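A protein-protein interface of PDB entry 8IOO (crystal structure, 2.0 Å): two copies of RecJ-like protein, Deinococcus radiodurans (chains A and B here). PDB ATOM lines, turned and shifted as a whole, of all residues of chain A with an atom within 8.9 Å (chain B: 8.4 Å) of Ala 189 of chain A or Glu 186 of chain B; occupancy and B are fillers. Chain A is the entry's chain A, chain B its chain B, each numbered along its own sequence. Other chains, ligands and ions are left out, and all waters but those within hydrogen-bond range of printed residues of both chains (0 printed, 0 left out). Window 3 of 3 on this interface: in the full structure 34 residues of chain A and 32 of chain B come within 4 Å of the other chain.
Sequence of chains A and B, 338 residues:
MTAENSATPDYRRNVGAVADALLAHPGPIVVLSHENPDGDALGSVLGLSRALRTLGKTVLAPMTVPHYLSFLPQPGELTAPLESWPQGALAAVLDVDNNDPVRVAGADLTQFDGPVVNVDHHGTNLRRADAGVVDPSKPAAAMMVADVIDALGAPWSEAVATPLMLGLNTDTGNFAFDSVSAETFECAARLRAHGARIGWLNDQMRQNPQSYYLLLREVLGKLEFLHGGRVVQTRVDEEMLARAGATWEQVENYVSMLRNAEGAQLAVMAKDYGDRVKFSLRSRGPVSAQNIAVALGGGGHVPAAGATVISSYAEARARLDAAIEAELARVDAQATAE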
ATOM      1  N   ALA A 161       7.694  23.423   3.265  1.00  0.00           N
ATOM      2  CA  ALA A 161       7.200  22.279   2.505  1.00  0.00           C
ATOM      3  C   ALA A 161       6.123  22.683   1.507  1.00  0.00           C
ATOM      4  O   ALA A 161       6.100  22.185   0.377  1.00  0.00           O
ATOM      5  CB  ALA A 161       6.677  21.218   3.481  1.00  0.00           C
ATOM      6  N   MET A 165       5.753  21.697  -2.497  1.00  0.00           N
ATOM      7  CA  MET A 165       4.637  20.817  -2.930  1.00  0.00           C
ATOM      8  C   MET A 165       3.933  21.417  -4.154  1.00  0.00           C
ATOM      9  O   MET A 165       3.562  20.657  -5.043  1.00  0.00           O
ATOM     10  CB  MET A 165       3.613  20.627  -1.812  1.00  0.00           C
ATOM     11  CG  MET A 165       2.372  19.874  -2.236  1.00  0.00           C
ATOM     12  SD  MET A 165       2.742  18.186  -2.741  1.00  0.00           S
ATOM     13  CE  MET A 165       2.582  17.341  -1.171  1.00  0.00           C
ATOM     14  N   LEU A 168       6.021  20.818  -7.220  1.00  0.00           N
ATOM     15  CA  LEU A 168       5.844  19.415  -7.591  1.00  0.00           C
ATOM     16  C   LEU A 168       4.527  19.178  -8.316  1.00  0.00           C
ATOM     17  O   LEU A 168       4.494  18.487  -9.349  1.00  0.00           O
ATOM     18  CB  LEU A 168       5.962  18.533  -6.342  1.00  0.00           C
ATOM     19  CG  LEU A 168       6.248  17.036  -6.494  1.00  0.00           C
ATOM     20  CD1 LEU A 168       7.562  16.817  -7.165  1.00  0.00           C
ATOM     21  CD2 LEU A 168       6.336  16.404  -5.096  1.00  0.00           C
ATOM     22  N   PHE A 175       0.573  15.294 -10.610  1.00  0.00           N
ATOM     23  CA  PHE A 175       1.009  13.897 -10.561  1.00  0.00           C
ATOM     24  C   PHE A 175       0.338  13.072 -11.665  1.00  0.00           C
ATOM     25  O   PHE A 175       0.048  11.892 -11.496  1.00  0.00           O
ATOM     26  CB  PHE A 175       0.751  13.301  -9.172  1.00  0.00           C
ATOM     27  CG  PHE A 175       1.400  14.083  -8.061  1.00  0.00           C
ATOM     28  CD1 PHE A 175       2.738  13.907  -7.755  1.00  0.00           C
ATOM     29  CD2 PHE A 175       0.670  15.018  -7.345  1.00  0.00           C
ATOM     30  CE1 PHE A 175       3.336  14.647  -6.737  1.00  0.00           C
ATOM     31  CE2 PHE A 175       1.252  15.744  -6.335  1.00  0.00           C
ATOM     32  CZ  PHE A 175       2.586  15.570  -6.029  1.00  0.00           C
ATOM     33  N   ALA A 182       8.138   6.766  -9.018  1.00  0.00           N
ATOM     34  CA  ALA A 182       7.903   6.385  -7.622  1.00  0.00           C
ATOM     35  C   ALA A 182       8.510   7.423  -6.674  1.00  0.00           C
ATOM     36  O   ALA A 182       7.873   7.854  -5.701  1.00  0.00           O
ATOM     37  CB  ALA A 182       8.464   4.985  -7.334  1.00  0.00           C
ATOM     38  N   GLU A 183       9.741   7.868  -6.963  1.00  0.00           N
ATOM     39  CA  GLU A 183      10.420   8.794  -6.062  1.00  0.00           C
ATOM     40  C   GLU A 183       9.767  10.181  -6.049  1.00  0.00           C
ATOM     41  O   GLU A 183       9.910  10.921  -5.075  1.00  0.00           O
ATOM     42  CB  GLU A 183      11.913   8.850  -6.452  1.00  0.00           C
ATOM     43  CG  GLU A 183      12.301   9.992  -7.342  1.00  0.00           C
ATOM     44  CD  GLU A 183      13.819  10.154  -7.480  1.00  0.00           C
ATOM     45  OE1 GLU A 183      14.511  10.170  -6.438  1.00  0.00           O
ATOM     46  OE2 GLU A 183      14.313  10.271  -8.620  1.00  0.00           O
ATOM     47  N   THR A 184       9.077  10.564  -7.127  1.00  0.00           N
ATOM     48  CA  THR A 184       8.217  11.753  -7.110  1.00  0.00           C
ATOM     49  C   THR A 184       7.143  11.657  -6.045  1.00  0.00           C
ATOM     50  O   THR A 184       6.901  12.609  -5.282  1.00  0.00           O
ATOM     51  CB  THR A 184       7.555  11.944  -8.482  1.00  0.00           C
ATOM     52  OG1 THR A 184       8.564  11.964  -9.487  1.00  0.00           O
ATOM     53  CG2 THR A 184       6.704  13.210  -8.549  1.00  0.00           C
ATOM     54  N   PHE A 185       6.481  10.503  -5.973  1.00  0.00           N
ATOM     55  CA  PHE A 185       5.447  10.344  -4.961  1.00  0.00           C
ATOM     56  C   PHE A 185       6.055  10.214  -3.587  1.00  0.00           C
ATOM     57  O   PHE A 185       5.480  10.708  -2.608  1.00  0.00           O
ATOM     58  CB  PHE A 185       4.572   9.124  -5.250  1.00  0.00           C
ATOM     59  CG  PHE A 185       3.527   9.344  -6.309  1.00  0.00           C
ATOM     60  CD1 PHE A 185       2.595  10.368  -6.181  1.00  0.00           C
ATOM     61  CD2 PHE A 185       3.436   8.496  -7.397  1.00  0.00           C
ATOM     62  CE1 PHE A 185       1.623  10.555  -7.141  1.00  0.00           C
ATOM     63  CE2 PHE A 185       2.465   8.680  -8.355  1.00  0.00           C
ATOM     64  CZ  PHE A 185       1.555   9.706  -8.225  1.00  0.00           C
ATOM     65  N   GLU A 186       7.230   9.593  -3.498  1.00  0.00           N
ATOM     66  CA  GLU A 186       7.924   9.524  -2.217  1.00  0.00           C
ATOM     67  C   GLU A 186       8.276  10.922  -1.726  1.00  0.00           C
ATOM     68  O   GLU A 186       8.201  11.205  -0.523  1.00  0.00           O
ATOM     69  CB  GLU A 186       9.174   8.661  -2.355  1.00  0.00           C
ATOM     70  CG  GLU A 186       8.900   7.178  -2.094  1.00  0.00           C
ATOM     71  CD  GLU A 186      10.054   6.294  -2.545  1.00  0.00           C
ATOM     72  OE1 GLU A 186      10.895   6.791  -3.321  1.00  0.00           O
ATOM     73  OE2 GLU A 186      10.110   5.117  -2.135  1.00  0.00           O
ATOM     74  N   CYS A 187       8.618  11.819  -2.657  1.00  0.00           N
ATOM     75  CA  CYS A 187       8.891  13.210  -2.296  1.00  0.00           C
ATOM     76  C   CYS A 187       7.635  13.934  -1.812  1.00  0.00           C
ATOM     77  O   CYS A 187       7.685  14.683  -0.832  1.00  0.00           O
ATOM     78  CB  CYS A 187       9.468  13.941  -3.500  1.00  0.00           C
ATOM     79  SG  CYS A 187       9.905  15.634  -3.111  1.00  0.00           S
ATOM     80  N   ALA A 188       6.505  13.739  -2.506  1.00  0.00           N
ATOM     81  CA  ALA A 188       5.233  14.306  -2.067  1.00  0.00           C
ATOM     82  C   ALA A 188       4.856  13.840  -0.668  1.00  0.00           C
ATOM     83  O   ALA A 188       4.396  14.632   0.164  1.00  0.00           O
ATOM     84  CB  ALA A 188       4.124  13.909  -3.040  1.00  0.00           C
ATOM     85  N   ALA A 189       4.973  12.541  -0.412  1.00  0.00           N
ATOM     86  CA  ALA A 189       4.673  12.025   0.922  1.00  0.00           C
ATOM     87  C   ALA A 189       5.476  12.748   1.984  1.00  0.00           C
ATOM     88  O   ALA A 189       4.934  13.161   3.017  1.00  0.00           O
ATOM     89  CB  ALA A 189       4.965  10.518   1.003  1.00  0.00           C
ATOM     90  N   ARG A 190       6.770  12.919   1.740  1.00  0.00           N
ATOM     91  CA  ARG A 190       7.650  13.564   2.704  1.00  0.00           C
ATOM     92  C   ARG A 190       7.263  15.032   2.914  1.00  0.00           C
ATOM     93  O   ARG A 190       7.194  15.511   4.053  1.00  0.00           O
ATOM     94  CB  ARG A 190       9.082  13.344   2.189  1.00  0.00           C
ATOM     95  CG  ARG A 190      10.063  12.853   3.183  1.00  0.00           C
ATOM     96  CD  ARG A 190      11.260  12.196   2.453  1.00  0.00           C
ATOM     97  NE  ARG A 190      11.697  12.801   1.198  1.00  0.00           N
ATOM     98  CZ  ARG A 190      11.886  12.109   0.077  1.00  0.00           C
ATOM     99  NH1 ARG A 190      11.652  10.804   0.015  1.00  0.00           N
ATOM    100  NH2 ARG A 190      12.327  12.738  -1.012  1.00  0.00           N
ATOM    101  N   LEU A 191       6.930  15.735   1.832  1.00  0.00           N
ATOM    102  CA  LEU A 191       6.463  17.113   1.921  1.00  0.00           C
ATOM    103  C   LEU A 191       5.146  17.195   2.689  1.00  0.00           C
ATOM    104  O   LEU A 191       4.979  18.051   3.574  1.00  0.00           O
ATOM    105  CB  LEU A 191       6.333  17.658   0.488  1.00  0.00           C
ATOM    106  CG  LEU A 191       7.639  17.825  -0.293  1.00  0.00           C
ATOM    107  CD1 LEU A 191       7.335  18.483  -1.630  1.00  0.00           C
ATOM    108  CD2 LEU A 191       8.506  18.800   0.517  1.00  0.00           C
ATOM    109  N   ARG A 192       4.209  16.290   2.392  1.00  0.00           N
ATOM    110  CA  ARG A 192       2.937  16.293   3.104  1.00  0.00           C
ATOM    111  C   ARG A 192       3.127  15.992   4.583  1.00  0.00           C
ATOM    112  O   ARG A 192       2.533  16.664   5.439  1.00  0.00           O
ATOM    113  CB  ARG A 192       1.956  15.331   2.426  1.00  0.00           C
ATOM    114  CG  ARG A 192       0.578  15.232   3.109  1.00  0.00           C
ATOM    115  CD  ARG A 192      -0.219  16.534   3.058  1.00  0.00           C
ATOM    116  NE  ARG A 192      -1.638  16.377   3.346  1.00  0.00           N
ATOM    117  CZ  ARG A 192      -2.427  17.375   3.716  1.00  0.00           C
ATOM    118  NH1 ARG A 192      -1.925  18.552   4.076  1.00  0.00           N
ATOM    119  NH2 ARG A 192      -3.740  17.171   3.797  1.00  0.00           N
ATOM    120  N   ALA A 193       4.011  15.043   4.910  1.00  0.00           N
ATOM    121  CA  ALA A 193       4.283  14.743   6.316  1.00  0.00           C
ATOM    122  C   ALA A 193       4.877  15.943   7.046  1.00  0.00           C
ATOM    123  O   ALA A 193       4.717  16.071   8.269  1.00  0.00           O
ATOM    124  CB  ALA A 193       5.238  13.551   6.432  1.00  0.00           C
ATOM    125  N   HIS A 194       5.567  16.822   6.320  1.00  0.00           N
ATOM    126  CA  HIS A 194       6.128  18.039   6.894  1.00  0.00           C
ATOM    127  C   HIS A 194       5.098  19.156   7.007  1.00  0.00           C
ATOM    128  O   HIS A 194       5.431  20.236   7.506  1.00  0.00           O
ATOM    129  CB  HIS A 194       7.302  18.494   6.020  1.00  0.00           C
ATOM    130  CG  HIS A 194       8.592  17.797   6.327  1.00  0.00           C
ATOM    131  ND1 HIS A 194       8.882  17.247   7.559  1.00  0.00           N
ATOM    132  CD2 HIS A 194       9.595  17.404   5.498  1.00  0.00           C
ATOM    133  CE1 HIS A 194      10.057  16.642   7.497  1.00  0.00           C
ATOM    134  NE2 HIS A 194      10.509  16.719   6.259  1.00  0.00           N
ATOM    135  N   GLY A 195       3.867  18.925   6.533  1.00  0.00           N
ATOM    136  CA  GLY A 195       2.787  19.880   6.660  1.00  0.00           C
ATOM    137  C   GLY A 195       2.366  20.650   5.423  1.00  0.00           C
ATOM    138  O   GLY A 195       1.543  21.562   5.538  1.00  0.00           O
ATOM    139  N   ALA A 196       2.902  20.308   4.249  1.00  0.00           N
ATOM    140  CA  ALA A 196       2.497  20.960   3.004  1.00  0.00           C
ATOM    141  C   ALA A 196       0.975  20.989   2.859  1.00  0.00           C
ATOM    142  O   ALA A 196       0.324  19.943   2.920  1.00  0.00           O
ATOM    143  CB  ALA A 196       3.127  20.212   1.815  1.00  0.00           C
ATOM    144  N   ILE A 198      -1.924  20.785   1.191  1.00  0.00           N
ATOM    145  CA  ILE A 198      -2.330  20.284  -0.116  1.00  0.00           C
ATOM    146  C   ILE A 198      -3.714  20.839  -0.498  1.00  0.00           C
ATOM    147  O   ILE A 198      -3.938  21.281  -1.635  1.00  0.00           O
ATOM    148  CB  ILE A 198      -2.303  18.748  -0.069  1.00  0.00           C
ATOM    149  CG1 ILE A 198      -2.754  18.132  -1.368  1.00  0.00           C
ATOM    150  CG2 ILE A 198      -3.251  18.259   0.973  1.00  0.00           C
ATOM    151  CD1 ILE A 198      -1.575  18.002  -2.225  1.00  0.00           C
ATOM    152  N   MET B 143      -6.622   1.891  -2.169  1.00  0.00           N
ATOM    153  CA  MET B 143      -5.462   1.849  -1.258  1.00  0.00           C
ATOM    154  C   MET B 143      -5.485   0.596  -0.397  1.00  0.00           C
ATOM    155  O   MET B 143      -4.470  -0.076  -0.166  1.00  0.00           O
ATOM    156  CB  MET B 143      -5.512   3.079  -0.308  1.00  0.00           C
ATOM    157  CG  MET B 143      -4.924   4.344  -0.838  1.00  0.00           C
ATOM    158  SD  MET B 143      -4.571   5.498   0.542  1.00  0.00           S
ATOM    159  CE  MET B 143      -3.643   4.578   1.745  1.00  0.00           C
ATOM    160  N   MET B 165      -4.385   2.588  -9.377  1.00  0.00           N
ATOM    161  CA  MET B 165      -3.925   3.974  -9.422  1.00  0.00           C
ATOM    162  C   MET B 165      -5.058   4.866  -9.902  1.00  0.00           C
ATOM    163  O   MET B 165      -5.229   6.003  -9.432  1.00  0.00           O
ATOM    164  CB  MET B 165      -2.733   4.096 -10.384  1.00  0.00           C
ATOM    165  CG  MET B 165      -2.187   5.494 -10.578  1.00  0.00           C
ATOM    166  SD  MET B 165      -1.394   6.148  -9.091  1.00  0.00           S
ATOM    167  CE  MET B 165       0.229   5.408  -9.333  1.00  0.00           C
ATOM    168  N   LEU B 168      -7.294   5.550  -6.994  1.00  0.00           N
ATOM    169  CA  LEU B 168      -6.596   6.483  -6.120  1.00  0.00           C
ATOM    170  C   LEU B 168      -6.706   7.907  -6.653  1.00  0.00           C
ATOM    171  O   LEU B 168      -7.011   8.842  -5.897  1.00  0.00           O
ATOM    172  CB  LEU B 168      -5.137   6.031  -5.981  1.00  0.00           C
ATOM    173  CG  LEU B 168      -4.293   6.638  -4.869  1.00  0.00           C
ATOM    174  CD1 LEU B 168      -4.983   6.412  -3.540  1.00  0.00           C
ATOM    175  CD2 LEU B 168      -2.875   6.041  -4.869  1.00  0.00           C
ATOM    176  N   PHE B 175      -5.034  13.909  -6.179  1.00  0.00           N
ATOM    177  CA  PHE B 175      -4.227  14.227  -5.004  1.00  0.00           C
ATOM    178  C   PHE B 175      -4.410  15.689  -4.580  1.00  0.00           C
ATOM    179  O   PHE B 175      -3.482  16.306  -4.063  1.00  0.00           O
ATOM    180  CB  PHE B 175      -2.750  13.906  -5.251  1.00  0.00           C
ATOM    181  CG  PHE B 175      -2.527  12.478  -5.649  1.00  0.00           C
ATOM    182  CD1 PHE B 175      -2.404  11.490  -4.693  1.00  0.00           C
ATOM    183  CD2 PHE B 175      -2.466  12.126  -6.990  1.00  0.00           C
ATOM    184  CE1 PHE B 175      -2.237  10.169  -5.070  1.00  0.00           C
ATOM    185  CE2 PHE B 175      -2.287  10.830  -7.371  1.00  0.00           C
ATOM    186  CZ  PHE B 175      -2.174   9.842  -6.415  1.00  0.00           C
ATOM    187  N   VAL B 180      -5.875  13.650   1.326  1.00  0.00           N
ATOM    188  CA  VAL B 180      -4.594  13.085   0.907  1.00  0.00           C
ATOM    189  C   VAL B 180      -3.595  13.190   2.058  1.00  0.00           C
ATOM    190  O   VAL B 180      -3.212  14.292   2.475  1.00  0.00           O
ATOM    191  CB  VAL B 180      -4.092  13.810  -0.348  1.00  0.00           C
ATOM    192  CG1 VAL B 180      -2.703  13.267  -0.799  1.00  0.00           C
ATOM    193  CG2 VAL B 180      -5.143  13.710  -1.445  1.00  0.00           C
ATOM    194  N   SER B 181      -3.164  12.044   2.582  1.00  0.00           N
ATOM    195  CA  SER B 181      -2.118  11.952   3.601  1.00  0.00           C
ATOM    196  C   SER B 181      -0.796  11.527   2.972  1.00  0.00           C
ATOM    197  O   SER B 181      -0.754  11.115   1.812  1.00  0.00           O
ATOM    198  CB  SER B 181      -2.475  10.901   4.642  1.00  0.00           C
ATOM    199  OG  SER B 181      -2.838   9.716   3.946  1.00  0.00           O
ATOM    200  N   ALA B 182       0.279  11.567   3.778  1.00  0.00           N
ATOM    201  CA  ALA B 182       1.565  11.029   3.339  1.00  0.00           C
ATOM    202  C   ALA B 182       1.421   9.570   2.915  1.00  0.00           C
ATOM    203  O   ALA B 182       2.063   9.108   1.967  1.00  0.00           O
ATOM    204  CB  ALA B 182       2.613  11.140   4.465  1.00  0.00           C
ATOM    205  N   GLU B 183       0.551   8.837   3.610  1.00  0.00           N
ATOM    206  CA  GLU B 183       0.331   7.431   3.292  1.00  0.00           C
ATOM    207  C   GLU B 183      -0.367   7.266   1.945  1.00  0.00           C
ATOM    208  O   GLU B 183      -0.124   6.289   1.217  1.00  0.00           O
ATOM    209  CB  GLU B 183      -0.456   6.789   4.441  1.00  0.00           C
ATOM    210  CG  GLU B 183      -1.442   5.726   4.092  1.00  0.00           C
ATOM    211  CD  GLU B 183      -2.077   5.096   5.331  1.00  0.00           C
ATOM    212  OE1 GLU B 183      -2.884   5.776   6.002  1.00  0.00           O
ATOM    213  OE2 GLU B 183      -1.771   3.914   5.627  1.00  0.00           O
ATOM    214  N   THR B 184      -1.185   8.240   1.562  1.00  0.00           N
ATOM    215  CA  THR B 184      -1.764   8.202   0.230  1.00  0.00           C
ATOM    216  C   THR B 184      -0.676   8.267  -0.834  1.00  0.00           C
ATOM    217  O   THR B 184      -0.701   7.506  -1.814  1.00  0.00           O
ATOM    218  CB  THR B 184      -2.761   9.343   0.067  1.00  0.00           C
ATOM    219  OG1 THR B 184      -3.779   9.264   1.072  1.00  0.00           O
ATOM    220  CG2 THR B 184      -3.386   9.312  -1.288  1.00  0.00           C
ATOM    221  N   PHE B 185       0.312   9.146  -0.635  1.00  0.00           N
ATOM    222  CA  PHE B 185       1.353   9.332  -1.637  1.00  0.00           C
ATOM    223  C   PHE B 185       2.269   8.122  -1.671  1.00  0.00           C
ATOM    224  O   PHE B 185       2.725   7.721  -2.740  1.00  0.00           O
ATOM    225  CB  PHE B 185       2.155  10.608  -1.331  1.00  0.00           C
ATOM    226  CG  PHE B 185       1.495  11.889  -1.821  1.00  0.00           C
ATOM    227  CD1 PHE B 185       1.018  12.026  -3.108  1.00  0.00           C
ATOM    228  CD2 PHE B 185       1.310  12.949  -0.943  1.00  0.00           C
ATOM    229  CE1 PHE B 185       0.400  13.212  -3.521  1.00  0.00           C
ATOM    230  CE2 PHE B 185       0.705  14.129  -1.353  1.00  0.00           C
ATOM    231  CZ  PHE B 185       0.251  14.260  -2.648  1.00  0.00           C
ATOM    232  N   GLU B 186       2.558   7.537  -0.504  1.00  0.00           N
ATOM    233  CA  GLU B 186       3.354   6.316  -0.467  1.00  0.00           C
ATOM    234  C   GLU B 186       2.673   5.184  -1.208  1.00  0.00           C
ATOM    235  O   GLU B 186       3.349   4.367  -1.842  1.00  0.00           O
ATOM    236  CB  GLU B 186       3.620   5.875   0.967  1.00  0.00           C
ATOM    237  CG  GLU B 186       4.585   6.775   1.714  1.00  0.00           C
ATOM    238  CD  GLU B 186       4.566   6.497   3.201  1.00  0.00           C
ATOM    239  OE1 GLU B 186       3.749   5.654   3.651  1.00  0.00           O
ATOM    240  OE2 GLU B 186       5.380   7.118   3.918  1.00  0.00           O
ATOM    241  N   CYS B 187       1.344   5.101  -1.126  1.00  0.00           N
ATOM    242  CA  CYS B 187       0.662   4.052  -1.857  1.00  0.00           C
ATOM    243  C   CYS B 187       0.793   4.300  -3.352  1.00  0.00           C
ATOM    244  O   CYS B 187       1.062   3.369  -4.128  1.00  0.00           O
ATOM    245  CB  CYS B 187      -0.814   3.965  -1.418  1.00  0.00           C
ATOM    246  SG  CYS B 187      -1.765   2.832  -2.420  1.00  0.00           S
ATOM    247  N   ALA B 188       0.689   5.565  -3.775  1.00  0.00           N
ATOM    248  CA  ALA B 188       0.853   5.853  -5.193  1.00  0.00           C
ATOM    249  C   ALA B 188       2.274   5.518  -5.650  1.00  0.00           C
ATOM    250  O   ALA B 188       2.469   4.990  -6.750  1.00  0.00           O
ATOM    251  CB  ALA B 188       0.514   7.316  -5.494  1.00  0.00           C
ATOM    252  N   ALA B 189       3.271   5.760  -4.791  1.00  0.00           N
ATOM    253  CA  ALA B 189       4.649   5.397  -5.139  1.00  0.00           C
ATOM    254  C   ALA B 189       4.788   3.890  -5.343  1.00  0.00           C
ATOM    255  O   ALA B 189       5.466   3.440  -6.279  1.00  0.00           O
ATOM    256  CB  ALA B 189       5.619   5.852  -4.041  1.00  0.00           C
ATOM    257  N   ARG B 190       4.189   3.092  -4.453  1.00  0.00           N
ATOM    258  CA  ARG B 190       4.213   1.638  -4.617  1.00  0.00           C
ATOM    259  C   ARG B 190       3.559   1.236  -5.927  1.00  0.00           C
ATOM    260  O   ARG B 190       4.139   0.482  -6.728  1.00  0.00           O
ATOM    261  CB  ARG B 190       3.512   0.965  -3.435  1.00  0.00           C
ATOM    262  CG  ARG B 190       4.211   1.266  -2.134  1.00  0.00           C
ATOM    263  CD  ARG B 190       3.715   0.366  -0.998  1.00  0.00           C
ATOM    264  NE  ARG B 190       4.185  -1.014  -1.084  1.00  0.00           N
ATOM    265  CZ  ARG B 190       5.309  -1.457  -0.532  1.00  0.00           C
ATOM    266  NH1 ARG B 190       6.161  -0.632   0.060  1.00  0.00           N
ATOM    267  NH2 ARG B 190       5.611  -2.756  -0.618  1.00  0.00           N
ATOM    268  N   LEU B 191       2.357   1.762  -6.180  1.00  0.00           N
ATOM    269  CA  LEU B 191       1.650   1.429  -7.409  1.00  0.00           C
ATOM    270  C   LEU B 191       2.461   1.767  -8.654  1.00  0.00           C
ATOM    271  O   LEU B 191       2.473   0.983  -9.615  1.00  0.00           O
ATOM    272  CB  LEU B 191       0.292   2.126  -7.448  1.00  0.00           C
ATOM    273  CG  LEU B 191      -0.638   1.532  -6.404  1.00  0.00           C
ATOM    274  CD1 LEU B 191      -1.957   2.285  -6.406  1.00  0.00           C
ATOM    275  CD2 LEU B 191      -0.882   0.030  -6.725  1.00  0.00           C
ATOM    276  N   ARG B 192       3.147   2.911  -8.663  1.00  0.00           N
ATOM    277  CA  ARG B 192       3.961   3.292  -9.815  1.00  0.00           C
ATOM    278  C   ARG B 192       5.143   2.348  -9.996  1.00  0.00           C
ATOM    279  O   ARG B 192       5.452   1.940 -11.122  1.00  0.00           O
ATOM    280  CB  ARG B 192       4.432   4.752  -9.657  1.00  0.00           C
ATOM    281  CG  ARG B 192       5.360   5.281 -10.747  1.00  0.00           C
ATOM    282  CD  ARG B 192       4.821   5.070 -12.158  1.00  0.00           C
ATOM    283  NE  ARG B 192       5.340   6.014 -13.140  1.00  0.00           N
ATOM    284  CZ  ARG B 192       4.797   6.214 -14.330  1.00  0.00           C
ATOM    285  NH1 ARG B 192       3.883   5.395 -14.814  1.00  0.00           N
ATOM    286  NH2 ARG B 192       5.242   7.207 -15.088  1.00  0.00           N
ATOM    287  N   ALA B 193       5.785   1.944  -8.894  1.00  0.00           N
ATOM    288  CA  ALA B 193       6.875   0.975  -8.976  1.00  0.00           C
ATOM    289  C   ALA B 193       6.398  -0.375  -9.516  1.00  0.00           C
ATOM    290  O   ALA B 193       7.128  -1.072 -10.252  1.00  0.00           O
ATOM    291  CB  ALA B 193       7.501   0.814  -7.587  1.00  0.00           C
ATOM    292  N   HIS B 194       5.181  -0.765  -9.166  1.00  0.00           N
ATOM    293  CA  HIS B 194       4.591  -1.972  -9.743  1.00  0.00           C
ATOM    294  C   HIS B 194       4.268  -1.821 -11.224  1.00  0.00           C
ATOM    295  O   HIS B 194       4.036  -2.832 -11.894  1.00  0.00           O
ATOM    296  CB  HIS B 194       3.328  -2.375  -8.961  1.00  0.00           C
ATOM    297  CG  HIS B 194       3.589  -2.836  -7.551  1.00  0.00           C
ATOM    298  ND1 HIS B 194       4.616  -3.694  -7.218  1.00  0.00           N
ATOM    299  CD2 HIS B 194       2.992  -2.502  -6.375  1.00  0.00           C
ATOM    300  CE1 HIS B 194       4.603  -3.917  -5.915  1.00  0.00           C
ATOM    301  NE2 HIS B 194       3.634  -3.200  -5.375  1.00  0.00           N
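Arg 192 of chain B touches Ala 182 of chain A (CG to N, 3.6 Å). CE1 of Phe 185 of chain A touches CE2 of Phe 175 of chain B, at 3.9 Å. Phe 185 of chain B touches Phe 185 of chain A (O to CB, 3.4 Å). Ala 188 of chain B touches Phe 185 of chain A (C to CD2, 3.6 Å). Phe 185 of chain A touches Ala 189 of chain B (CB to N, 3.6 Å). CG of Phe 185 of chain B touches CB of Ala 188 of chain A, at 3.5 Å. N of Ala 189 of chain A touches CB of Phe 185 of chain B (3.5 Å). Ala 189 of chain A touches Glu 186 of chain B (CB to CG, 3.8 Å). Ser 181 of chain B touches Arg 192 of chain A (C to CG, 3.95 Å). Arg 192 of chain A touches Ala 182 of chain B.
Of the printed residues of chain B, Ala 189 of chain A touches Ala 182 (3.4 Å), Phe 185 (3.5 Å) and Glu 186 (3.8 Å). Glu 186 of chain B touches one residue of chain A. Of the printed residues of chain A, Val 180 of chain B touches Arg 192. Of the printed residues of chain B, Arg 192 of chain A touches Val 180, Ser 181 and Ala 182. Of the printed residues of chain A, Ala 189 of chain B touches Ala 182 and Phe 185. Of the printed residues of chain A, Phe 185 of chain B touches Met 165, Phe 175, Phe 185, Ala 188 and Ala 189. The nearest residue of chain B that does not touch Ala 189 of chain A is Glu 183 of chain B (5.4 Å).
NE of Arg 192 of chain A lies within hydrogen-bond range of O of Val 180 of chain B (2.8 Å).
NH1 of Arg 192 of chain A is in hydrogen-bond range of O of Ala 196 of chain A, 2.9 Å away. The side-chain hydroxyl (OG1) of Thr 184 of chain B is in hydrogen-bond range of the side-chain hydroxyl (OG) of Ser 181 of chain B (3.1 Å).
Of the 20 printed residues of chain A, 8 touch a printed residue of chain B. Hydrophobic or aromatic side chains of chain A that line the printed part of chain B: Met 165, Phe 175, Ala 182, Phe 185, Ala 188, Ala 189 and Ile 198.
Ala 182 of chain A touches Ala 189 of chain B, and with the chains exchanged Ala 189 of chain A touches Ala 182 of chain B. Phe 185 of chain A touches its own counterpart, Phe 185 of chain B. Phe 185 of chain A touches Ala 188 of chain B, and with the chains exchanged Ala 188 of chain A touches Phe 185 of chain B. Phe 185 of chain A touches Ala 189 of chain B, and with the chains exchanged Ala 189 of chain A touches Phe 185 of chain B. Positions printed for both chains: 165, 168, 175, 182, 183, 184, 185, 186, 187, 188, 189, 190, 191, 192, 193 and 194. Of the 16 pairs that touch across the chains among the printed residues, 11 have their exchanged pair printed and touching as well.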
